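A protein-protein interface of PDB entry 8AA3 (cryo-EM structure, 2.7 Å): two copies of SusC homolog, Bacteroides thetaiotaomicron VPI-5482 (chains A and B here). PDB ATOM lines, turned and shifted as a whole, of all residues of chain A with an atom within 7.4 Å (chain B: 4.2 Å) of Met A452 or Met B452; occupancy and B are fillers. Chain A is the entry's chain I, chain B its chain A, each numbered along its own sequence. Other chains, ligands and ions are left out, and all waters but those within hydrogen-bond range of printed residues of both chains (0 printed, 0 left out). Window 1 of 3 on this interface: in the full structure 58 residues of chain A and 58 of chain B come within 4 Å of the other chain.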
ATOM      1  N   LEU A 196     -28.846   1.531 -12.050  1.00  0.00           N
ATOM      2  CA  LEU A 196     -28.120   2.558 -11.322  1.00  0.00           C
ATOM      3  C   LEU A 196     -28.355   3.918 -11.968  1.00  0.00           C
ATOM      4  O   LEU A 196     -28.688   4.021 -13.151  1.00  0.00           O
ATOM      5  CB  LEU A 196     -26.619   2.252 -11.281  1.00  0.00           C
ATOM      6  CG  LEU A 196     -26.187   0.984 -10.542  1.00  0.00           C
ATOM      7  CD1 LEU A 196     -24.847   0.492 -11.064  1.00  0.00           C
ATOM      8  CD2 LEU A 196     -26.122   1.233  -9.043  1.00  0.00           C
ATOM      9  N   PHE A 388     -22.049   5.778  -1.465  1.00  0.00           N
ATOM     10  CA  PHE A 388     -23.180   4.883  -1.293  1.00  0.00           C
ATOM     11  C   PHE A 388     -24.295   5.271  -2.251  1.00  0.00           C
ATOM     12  O   PHE A 388     -24.490   6.449  -2.555  1.00  0.00           O
ATOM     13  CB  PHE A 388     -23.694   4.920   0.153  1.00  0.00           C
ATOM     14  CG  PHE A 388     -24.911   4.076   0.385  1.00  0.00           C
ATOM     15  CD1 PHE A 388     -24.794   2.724   0.654  1.00  0.00           C
ATOM     16  CD2 PHE A 388     -26.176   4.639   0.337  1.00  0.00           C
ATOM     17  CE1 PHE A 388     -25.915   1.951   0.868  1.00  0.00           C
ATOM     18  CE2 PHE A 388     -27.299   3.871   0.545  1.00  0.00           C
ATOM     19  CZ  PHE A 388     -27.169   2.527   0.814  1.00  0.00           C
ATOM     20  N   THR A 389     -25.024   4.265  -2.727  1.00  0.00           N
ATOM     21  CA  THR A 389     -26.212   4.515  -3.526  1.00  0.00           C
ATOM     22  C   THR A 389     -27.229   3.405  -3.297  1.00  0.00           C
ATOM     23  O   THR A 389     -26.874   2.233  -3.113  1.00  0.00           O
ATOM     24  CB  THR A 389     -25.883   4.655  -5.022  1.00  0.00           C
ATOM     25  OG1 THR A 389     -27.025   5.172  -5.716  1.00  0.00           O
ATOM     26  CG2 THR A 389     -25.494   3.323  -5.630  1.00  0.00           C
ATOM     27  N   LEU A 390     -28.497   3.806  -3.283  1.00  0.00           N
ATOM     28  CA  LEU A 390     -29.635   2.912  -3.140  1.00  0.00           C
ATOM     29  C   LEU A 390     -30.566   3.122  -4.323  1.00  0.00           C
ATOM     30  O   LEU A 390     -30.870   4.265  -4.682  1.00  0.00           O
ATOM     31  CB  LEU A 390     -30.382   3.169  -1.829  1.00  0.00           C
ATOM     32  CG  LEU A 390     -31.696   2.401  -1.671  1.00  0.00           C
ATOM     33  CD1 LEU A 390     -31.442   0.904  -1.635  1.00  0.00           C
ATOM     34  CD2 LEU A 390     -32.452   2.864  -0.436  1.00  0.00           C
ATOM     35  N   ASN A 391     -31.014   2.024  -4.924  1.00  0.00           N
ATOM     36  CA  ASN A 391     -31.876   2.079  -6.093  1.00  0.00           C
ATOM     37  C   ASN A 391     -33.082   1.178  -5.886  1.00  0.00           C
ATOM     38  O   ASN A 391     -32.970   0.105  -5.291  1.00  0.00           O
ATOM     39  CB  ASN A 391     -31.119   1.660  -7.357  1.00  0.00           C
ATOM     40  CG  ASN A 391     -29.943   2.568  -7.658  1.00  0.00           C
ATOM     41  OD1 ASN A 391     -30.096   3.614  -8.288  1.00  0.00           O
ATOM     42  ND2 ASN A 391     -28.760   2.174  -7.203  1.00  0.00           N
ATOM     43  N   TYR A 449     -36.928  -4.421  -7.585  1.00  0.00           N
ATOM     44  CA  TYR A 449     -35.502  -4.693  -7.470  1.00  0.00           C
ATOM     45  C   TYR A 449     -34.853  -3.589  -6.650  1.00  0.00           C
ATOM     46  O   TYR A 449     -34.858  -2.424  -7.059  1.00  0.00           O
ATOM     47  CB  TYR A 449     -34.861  -4.788  -8.860  1.00  0.00           C
ATOM     48  CG  TYR A 449     -33.389  -5.128  -8.865  1.00  0.00           C
ATOM     49  CD1 TYR A 449     -32.959  -6.448  -8.840  1.00  0.00           C
ATOM     50  CD2 TYR A 449     -32.427  -4.128  -8.915  1.00  0.00           C
ATOM     51  CE1 TYR A 449     -31.613  -6.762  -8.854  1.00  0.00           C
ATOM     52  CE2 TYR A 449     -31.080  -4.432  -8.927  1.00  0.00           C
ATOM     53  CZ  TYR A 449     -30.678  -5.749  -8.897  1.00  0.00           C
ATOM     54  OH  TYR A 449     -29.336  -6.051  -8.913  1.00  0.00           O
ATOM     55  N   TRP A 450     -34.304  -3.959  -5.499  1.00  0.00           N
ATOM     56  CA  TRP A 450     -33.553  -3.051  -4.644  1.00  0.00           C
ATOM     57  C   TRP A 450     -32.063  -3.298  -4.843  1.00  0.00           C
ATOM     58  O   TRP A 450     -31.592  -4.429  -4.695  1.00  0.00           O
ATOM     59  CB  TRP A 450     -33.925  -3.247  -3.173  1.00  0.00           C
ATOM     60  CG  TRP A 450     -35.283  -2.734  -2.805  1.00  0.00           C
ATOM     61  CD1 TRP A 450     -36.470  -3.397  -2.924  1.00  0.00           C
ATOM     62  CD2 TRP A 450     -35.594  -1.455  -2.238  1.00  0.00           C
ATOM     63  NE1 TRP A 450     -37.501  -2.607  -2.475  1.00  0.00           N
ATOM     64  CE2 TRP A 450     -36.989  -1.411  -2.048  1.00  0.00           C
ATOM     65  CE3 TRP A 450     -34.828  -0.343  -1.876  1.00  0.00           C
ATOM     66  CZ2 TRP A 450     -37.634  -0.297  -1.512  1.00  0.00           C
ATOM     67  CZ3 TRP A 450     -35.470   0.761  -1.345  1.00  0.00           C
ATOM     68  CH2 TRP A 450     -36.859   0.776  -1.169  1.00  0.00           C
ATOM     69  N   ARG A 451     -31.331  -2.240  -5.176  1.00  0.00           N
ATOM     70  CA  ARG A 451     -29.893  -2.309  -5.398  1.00  0.00           C
ATOM     71  C   ARG A 451     -29.180  -1.491  -4.332  1.00  0.00           C
ATOM     72  O   ARG A 451     -29.570  -0.353  -4.050  1.00  0.00           O
ATOM     73  CB  ARG A 451     -29.517  -1.809  -6.796  1.00  0.00           C
ATOM     74  CG  ARG A 451     -28.022  -1.856  -7.074  1.00  0.00           C
ATOM     75  CD  ARG A 451     -27.599  -3.228  -7.576  1.00  0.00           C
ATOM     76  NE  ARG A 451     -26.170  -3.292  -7.862  1.00  0.00           N
ATOM     77  CZ  ARG A 451     -25.607  -2.861  -8.982  1.00  0.00           C
ATOM     78  NH1 ARG A 451     -26.326  -2.336  -9.960  1.00  0.00           N
ATOM     79  NH2 ARG A 451     -24.289  -2.963  -9.127  1.00  0.00           N
ATOM     80  N   MET A 452     -28.127  -2.075  -3.762  1.00  0.00           N
ATOM     81  CA  MET A 452     -27.365  -1.500  -2.661  1.00  0.00           C
ATOM     82  C   MET A 452     -25.910  -1.485  -3.096  1.00  0.00           C
ATOM     83  O   MET A 452     -25.288  -2.548  -3.182  1.00  0.00           O
ATOM     84  CB  MET A 452     -27.516  -2.354  -1.403  1.00  0.00           C
ATOM     85  CG  MET A 452     -26.967  -1.740  -0.140  1.00  0.00           C
ATOM     86  SD  MET A 452     -28.203  -0.663   0.576  1.00  0.00           S
ATOM     87  CE  MET A 452     -29.337  -1.927   1.136  1.00  0.00           C
ATOM     88  N   PHE A 453     -25.356  -0.307  -3.367  1.00  0.00           N
ATOM     89  CA  PHE A 453     -23.966  -0.215  -3.809  1.00  0.00           C
ATOM     90  C   PHE A 453     -23.232   0.734  -2.869  1.00  0.00           C
ATOM     91  O   PHE A 453     -23.340   1.955  -3.003  1.00  0.00           O
ATOM     92  CB  PHE A 453     -23.888   0.248  -5.259  1.00  0.00           C
ATOM     93  CG  PHE A 453     -22.494   0.319  -5.799  1.00  0.00           C
ATOM     94  CD1 PHE A 453     -21.814  -0.834  -6.152  1.00  0.00           C
ATOM     95  CD2 PHE A 453     -21.859   1.540  -5.953  1.00  0.00           C
ATOM     96  CE1 PHE A 453     -20.530  -0.771  -6.651  1.00  0.00           C
ATOM     97  CE2 PHE A 453     -20.575   1.608  -6.449  1.00  0.00           C
ATOM     98  CZ  PHE A 453     -19.910   0.452  -6.799  1.00  0.00           C
ATOM     99  N   GLY A 454     -22.487   0.176  -1.917  1.00  0.00           N
ATOM    100  CA  GLY A 454     -21.787   0.993  -0.946  1.00  0.00           C
ATOM    101  C   GLY A 454     -20.300   0.718  -0.891  1.00  0.00           C
ATOM    102  O   GLY A 454     -19.848  -0.365  -1.270  1.00  0.00           O
ATOM    103  N   LEU A 474     -19.545  -3.195  -0.888  1.00  0.00           N
ATOM    104  CA  LEU A 474     -20.679  -4.093  -0.730  1.00  0.00           C
ATOM    105  C   LEU A 474     -21.693  -3.842  -1.836  1.00  0.00           C
ATOM    106  O   LEU A 474     -21.987  -2.691  -2.175  1.00  0.00           O
ATOM    107  CB  LEU A 474     -21.344  -3.912   0.642  1.00  0.00           C
ATOM    108  CG  LEU A 474     -22.607  -4.730   0.919  1.00  0.00           C
ATOM    109  CD1 LEU A 474     -22.273  -6.209   1.042  1.00  0.00           C
ATOM    110  CD2 LEU A 474     -23.309  -4.229   2.173  1.00  0.00           C
ATOM    111  N   ASP A 475     -22.223  -4.930  -2.394  1.00  0.00           N
ATOM    112  CA  ASP A 475     -23.267  -4.883  -3.413  1.00  0.00           C
ATOM    113  C   ASP A 475     -24.343  -5.888  -3.024  1.00  0.00           C
ATOM    114  O   ASP A 475     -24.116  -7.101  -3.084  1.00  0.00           O
ATOM    115  CB  ASP A 475     -22.705  -5.189  -4.802  1.00  0.00           C
ATOM    116  CG  ASP A 475     -23.687  -4.865  -5.912  1.00  0.00           C
ATOM    117  OD1 ASP A 475     -24.738  -4.257  -5.622  1.00  0.00           O
ATOM    118  OD2 ASP A 475     -23.407  -5.219  -7.078  1.00  0.00           O
ATOM    119  N   TYR A 476     -25.504  -5.384  -2.621  1.00  0.00           N
ATOM    120  CA  TYR A 476     -26.616  -6.214  -2.170  1.00  0.00           C
ATOM    121  C   TYR A 476     -27.809  -5.989  -3.086  1.00  0.00           C
ATOM    122  O   TYR A 476     -28.316  -4.868  -3.189  1.00  0.00           O
ATOM    123  CB  TYR A 476     -26.984  -5.898  -0.719  1.00  0.00           C
ATOM    124  CG  TYR A 476     -28.237  -6.594  -0.237  1.00  0.00           C
ATOM    125  CD1 TYR A 476     -28.311  -7.980  -0.194  1.00  0.00           C
ATOM    126  CD2 TYR A 476     -29.344  -5.864   0.177  1.00  0.00           C
ATOM    127  CE1 TYR A 476     -29.455  -8.620   0.246  1.00  0.00           C
ATOM    128  CE2 TYR A 476     -30.491  -6.497   0.618  1.00  0.00           C
ATOM    129  CZ  TYR A 476     -30.540  -7.874   0.650  1.00  0.00           C
ATOM    130  OH  TYR A 476     -31.680  -8.508   1.089  1.00  0.00           O
ATOM    131  N   ALA A 477     -28.265  -7.052  -3.739  1.00  0.00           N
ATOM    132  CA  ALA A 477     -29.367  -6.980  -4.685  1.00  0.00           C
ATOM    133  C   ALA A 477     -30.515  -7.849  -4.194  1.00  0.00           C
ATOM    134  O   ALA A 477     -30.313  -9.019  -3.856  1.00  0.00           O
ATOM    135  CB  ALA A 477     -28.920  -7.421  -6.080  1.00  0.00           C
ATOM    136  N   ASN A 478     -31.712  -7.272  -4.158  1.00  0.00           N
ATOM    137  CA  ASN A 478     -32.923  -7.956  -3.732  1.00  0.00           C
ATOM    138  C   ASN A 478     -33.940  -7.881  -4.860  1.00  0.00           C
ATOM    139  O   ASN A 478     -34.152  -6.810  -5.432  1.00  0.00           O
ATOM    140  CB  ASN A 478     -33.485  -7.321  -2.455  1.00  0.00           C
ATOM    141  CG  ASN A 478     -34.727  -8.022  -1.943  1.00  0.00           C
ATOM    142  OD1 ASN A 478     -35.124  -9.067  -2.455  1.00  0.00           O
ATOM    143  ND2 ASN A 478     -35.354  -7.441  -0.928  1.00  0.00           N
ATOM    144  N   TRP A 508     -28.711 -11.421  -3.865  1.00  0.00           N
ATOM    145  CA  TRP A 508     -27.315 -11.451  -4.279  1.00  0.00           C
ATOM    146  C   TRP A 508     -26.521 -10.599  -3.302  1.00  0.00           C
ATOM    147  O   TRP A 508     -26.940  -9.487  -2.972  1.00  0.00           O
ATOM    148  CB  TRP A 508     -27.137 -10.918  -5.707  1.00  0.00           C
ATOM    149  CG  TRP A 508     -27.855 -11.703  -6.767  1.00  0.00           C
ATOM    150  CD1 TRP A 508     -27.378 -12.784  -7.447  1.00  0.00           C
ATOM    151  CD2 TRP A 508     -29.168 -11.453  -7.284  1.00  0.00           C
ATOM    152  NE1 TRP A 508     -28.314 -13.230  -8.346  1.00  0.00           N
ATOM    153  CE2 TRP A 508     -29.423 -12.429  -8.267  1.00  0.00           C
ATOM    154  CE3 TRP A 508     -30.156 -10.503  -7.006  1.00  0.00           C
ATOM    155  CZ2 TRP A 508     -30.621 -12.482  -8.974  1.00  0.00           C
ATOM    156  CZ3 TRP A 508     -31.345 -10.557  -7.710  1.00  0.00           C
ATOM    157  CH2 TRP A 508     -31.567 -11.539  -8.683  1.00  0.00           C
ATOM    158  N   LYS A 510     -22.452  -9.430  -2.633  1.00  0.00           N
ATOM    159  CA  LYS A 510     -21.036  -9.406  -2.966  1.00  0.00           C
ATOM    160  C   LYS A 510     -20.325  -8.467  -2.006  1.00  0.00           C
ATOM    161  O   LYS A 510     -20.792  -7.348  -1.770  1.00  0.00           O
ATOM    162  CB  LYS A 510     -20.816  -8.944  -4.410  1.00  0.00           C
ATOM    163  CG  LYS A 510     -21.401  -9.870  -5.457  1.00  0.00           C
ATOM    164  CD  LYS A 510     -21.087  -9.386  -6.861  1.00  0.00           C
ATOM    165  CE  LYS A 510     -21.870  -8.128  -7.199  1.00  0.00           C
ATOM    166  NZ  LYS A 510     -23.334  -8.389  -7.270  1.00  0.00           N
ATOM    167  N   PHE B 388     -29.507   9.030   6.741  1.00  0.00           N
ATOM    168  CA  PHE B 388     -29.706   7.681   6.243  1.00  0.00           C
ATOM    169  C   PHE B 388     -28.946   6.693   7.113  1.00  0.00           C
ATOM    170  O   PHE B 388     -27.871   6.998   7.632  1.00  0.00           O
ATOM    171  CB  PHE B 388     -29.240   7.561   4.784  1.00  0.00           C
ATOM    172  CG  PHE B 388     -29.345   6.174   4.226  1.00  0.00           C
ATOM    173  CD1 PHE B 388     -30.536   5.713   3.694  1.00  0.00           C
ATOM    174  CD2 PHE B 388     -28.247   5.329   4.234  1.00  0.00           C
ATOM    175  CE1 PHE B 388     -30.628   4.435   3.182  1.00  0.00           C
ATOM    176  CE2 PHE B 388     -28.335   4.053   3.728  1.00  0.00           C
ATOM    177  CZ  PHE B 388     -29.525   3.606   3.198  1.00  0.00           C
ATOM    178  N   THR B 389     -29.518   5.501   7.269  1.00  0.00           N
ATOM    179  CA  THR B 389     -28.821   4.420   7.947  1.00  0.00           C
ATOM    180  C   THR B 389     -29.254   3.083   7.361  1.00  0.00           C
ATOM    181  O   THR B 389     -30.417   2.892   6.979  1.00  0.00           O
ATOM    182  CB  THR B 389     -29.050   4.450   9.467  1.00  0.00           C
ATOM    183  OG1 THR B 389     -28.133   3.553  10.106  1.00  0.00           O
ATOM    184  CG2 THR B 389     -30.466   4.047   9.822  1.00  0.00           C
ATOM    185  N   LEU B 390     -28.287   2.175   7.272  1.00  0.00           N
ATOM    186  CA  LEU B 390     -28.484   0.813   6.801  1.00  0.00           C
ATOM    187  C   LEU B 390     -27.996  -0.145   7.874  1.00  0.00           C
ATOM    188  O   LEU B 390     -26.906   0.038   8.427  1.00  0.00           O
ATOM    189  CB  LEU B 390     -27.733   0.564   5.490  1.00  0.00           C
ATOM    190  CG  LEU B 390     -27.733  -0.888   5.009  1.00  0.00           C
ATOM    191  CD1 LEU B 390     -29.146  -1.347   4.687  1.00  0.00           C
ATOM    192  CD2 LEU B 390     -26.808  -1.066   3.815  1.00  0.00           C
ATOM    193  N   ARG B 451     -32.358  -3.442   7.467  1.00  0.00           N
ATOM    194  CA  ARG B 451     -33.148  -2.281   7.848  1.00  0.00           C
ATOM    195  C   ARG B 451     -32.658  -1.063   7.079  1.00  0.00           C
ATOM    196  O   ARG B 451     -31.449  -0.819   6.997  1.00  0.00           O
ATOM    197  CB  ARG B 451     -33.076  -2.023   9.356  1.00  0.00           C
ATOM    198  CG  ARG B 451     -33.882  -0.814   9.804  1.00  0.00           C
ATOM    199  CD  ARG B 451     -35.338  -1.182  10.052  1.00  0.00           C
ATOM    200  NE  ARG B 451     -36.127  -0.040  10.496  1.00  0.00           N
ATOM    201  CZ  ARG B 451     -36.171   0.406  11.744  1.00  0.00           C
ATOM    202  NH1 ARG B 451     -35.490  -0.183  12.712  1.00  0.00           N
ATOM    203  NH2 ARG B 451     -36.921   1.466  12.028  1.00  0.00           N
ATOM    204  N   MET B 452     -33.604  -0.301   6.535  1.00  0.00           N
ATOM    205  CA  MET B 452     -33.342   0.854   5.685  1.00  0.00           C
ATOM    206  C   MET B 452     -34.095   2.024   6.294  1.00  0.00           C
ATOM    207  O   MET B 452     -35.327   2.057   6.230  1.00  0.00           O
ATOM    208  CB  MET B 452     -33.848   0.600   4.267  1.00  0.00           C
ATOM    209  CG  MET B 452     -33.428   1.623   3.241  1.00  0.00           C
ATOM    210  SD  MET B 452     -31.804   1.202   2.620  1.00  0.00           S
ATOM    211  CE  MET B 452     -32.269  -0.236   1.668  1.00  0.00           C
ATOM    212  N   PHE B 453     -33.383   2.985   6.876  1.00  0.00           N
ATOM    213  CA  PHE B 453     -34.038   4.133   7.499  1.00  0.00           C
ATOM    214  C   PHE B 453     -33.460   5.401   6.882  1.00  0.00           C
ATOM    215  O   PHE B 453     -32.370   5.838   7.258  1.00  0.00           O
ATOM    216  CB  PHE B 453     -33.859   4.104   9.012  1.00  0.00           C
ATOM    217  CG  PHE B 453     -34.547   5.227   9.726  1.00  0.00           C
ATOM    218  CD1 PHE B 453     -35.920   5.210   9.909  1.00  0.00           C
ATOM    219  CD2 PHE B 453     -33.823   6.300  10.214  1.00  0.00           C
ATOM    220  CE1 PHE B 453     -36.557   6.240  10.567  1.00  0.00           C
ATOM    221  CE2 PHE B 453     -34.454   7.335  10.872  1.00  0.00           C
ATOM    222  CZ  PHE B 453     -35.821   7.304  11.049  1.00  0.00           C
ATOM    223  N   GLY B 454     -34.187   5.991   5.934  1.00  0.00           N
ATOM    224  CA  GLY B 454     -33.701   7.176   5.255  1.00  0.00           C
ATOM    225  C   GLY B 454     -34.658   8.346   5.330  1.00  0.00           C
ATOM    226  O   GLY B 454     -35.862   8.158   5.525  1.00  0.00           O
ATOM    227  N   LEU B 474     -38.405   7.205   4.591  1.00  0.00           N
ATOM    228  CA  LEU B 474     -38.607   5.849   4.105  1.00  0.00           C
ATOM    229  C   LEU B 474     -38.033   4.854   5.103  1.00  0.00           C
ATOM    230  O   LEU B 474     -36.938   5.055   5.640  1.00  0.00           O
ATOM    231  CB  LEU B 474     -37.952   5.650   2.731  1.00  0.00           C
ATOM    232  CG  LEU B 474     -38.007   4.244   2.129  1.00  0.00           C
ATOM    233  CD1 LEU B 474     -39.431   3.880   1.739  1.00  0.00           C
ATOM    234  CD2 LEU B 474     -37.073   4.134   0.934  1.00  0.00           C
ATOM    235  N   ASP B 475     -38.783   3.780   5.346  1.00  0.00           N
ATOM    236  CA  ASP B 475     -38.360   2.683   6.212  1.00  0.00           C
ATOM    237  C   ASP B 475     -38.653   1.377   5.486  1.00  0.00           C
ATOM    238  O   ASP B 475     -39.818   1.004   5.315  1.00  0.00           O
ATOM    239  CB  ASP B 475     -39.074   2.733   7.563  1.00  0.00           C
ATOM    240  CG  ASP B 475     -38.454   1.798   8.585  1.00  0.00           C
ATOM    241  OD1 ASP B 475     -37.379   1.230   8.301  1.00  0.00           O
ATOM    242  OD2 ASP B 475     -39.042   1.630   9.674  1.00  0.00           O
ATOM    243  N   TYR B 476     -37.600   0.690   5.056  1.00  0.00           N
ATOM    244  CA  TYR B 476     -37.716  -0.553   4.303  1.00  0.00           C
ATOM    245  C   TYR B 476     -37.054  -1.675   5.089  1.00  0.00           C
ATOM    246  O   TYR B 476     -35.852  -1.621   5.363  1.00  0.00           O
ATOM    247  CB  TYR B 476     -37.081  -0.418   2.918  1.00  0.00           C
ATOM    248  CG  TYR B 476     -37.009  -1.715   2.146  1.00  0.00           C
ATOM    249  CD1 TYR B 476     -38.163  -2.406   1.800  1.00  0.00           C
ATOM    250  CD2 TYR B 476     -35.786  -2.249   1.760  1.00  0.00           C
ATOM    251  CE1 TYR B 476     -38.102  -3.591   1.094  1.00  0.00           C
ATOM    252  CE2 TYR B 476     -35.715  -3.435   1.054  1.00  0.00           C
ATOM    253  CZ  TYR B 476     -36.876  -4.102   0.723  1.00  0.00           C
ATOM    254  OH  TYR B 476     -36.812  -5.282   0.021  1.00  0.00           O
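ND2 of Asn A478 lies within hydrogen-bond range of OH of Tyr B476, 2.8 Å away.
Phe B388 touches its own counterpart, Phe A388. Leu A390 touches Met B452, and with the chains exchanged Met A452 touches Leu B390. Met A452 touches its own counterpart, Met B452. 10 positions are printed for both chains. Of the 7 pairs that touch across the chains among the printed residues, 4 have their exchanged pair printed and touching as well.
The backbone carbonyl oxygen of Asn A478 lies within hydrogen-bond range of the backbone NH of Trp A450 (2.9 Å). The backbone NH (N) of Met A452 lies within hydrogen-bond range of the backbone carbonyl oxygen (O) of Tyr A476. N of Met B452 sits at hydrogen-bond distance from O of Tyr B476, 2.9 Å away. O of Gly B454 lies within hydrogen-bond range of N of Leu B474, at 2.9 Å.
Phe B388 touches Phe A388. Leu A390 touches Met B452 (CD2 to SD, 3.5 Å). CH2 of Trp A450 touches CD2 of Leu B474 (3.97 Å). Tyr B476 touches Trp A450 (OH to CD1, 3.5 Å). Leu B390 touches Met A452 (CD2 to SD, 3.5 Å). CE of Met A452 touches CE of Met B452 (3.4 Å).
Of the printed residues of chain A, Met B452 touches Leu A390 and Met A452. Of the printed residues of chain B, Trp A450 touches Leu B474 (3.97 Å) and Tyr B476 (3.5 Å). Of the printed residues of chain B, Leu A390 touches Met B452. Printed residues of chain B within 4 Å of Asn A478: Tyr B476. Of the printed residues of chain B, Phe A388 touches Phe B388 (3.4 Å). Printed residues of chain A within 4 Å of Leu B390: Met A452. Asn A391 touches none of the printed residues of chain B. The nearest residue of chain A that does not touch Met B452 is Trp A450 (4.4 Å).
Of the 10 printed residues of chain B, 5 touch a printed residue of chain A. Of the 18 printed residues of chain A, 5 touch a printed residue of chain B. Hydrophobic or aromatic side chains of chain A within 4 Å of the printed part of chain B: Phe A388, Leu A390, Trp A450 and Met A452. Among the printed residues, no Asp or Glu carboxylate lies within 4 Å of a Lys or Arg side-chain nitrogen of the other chain.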
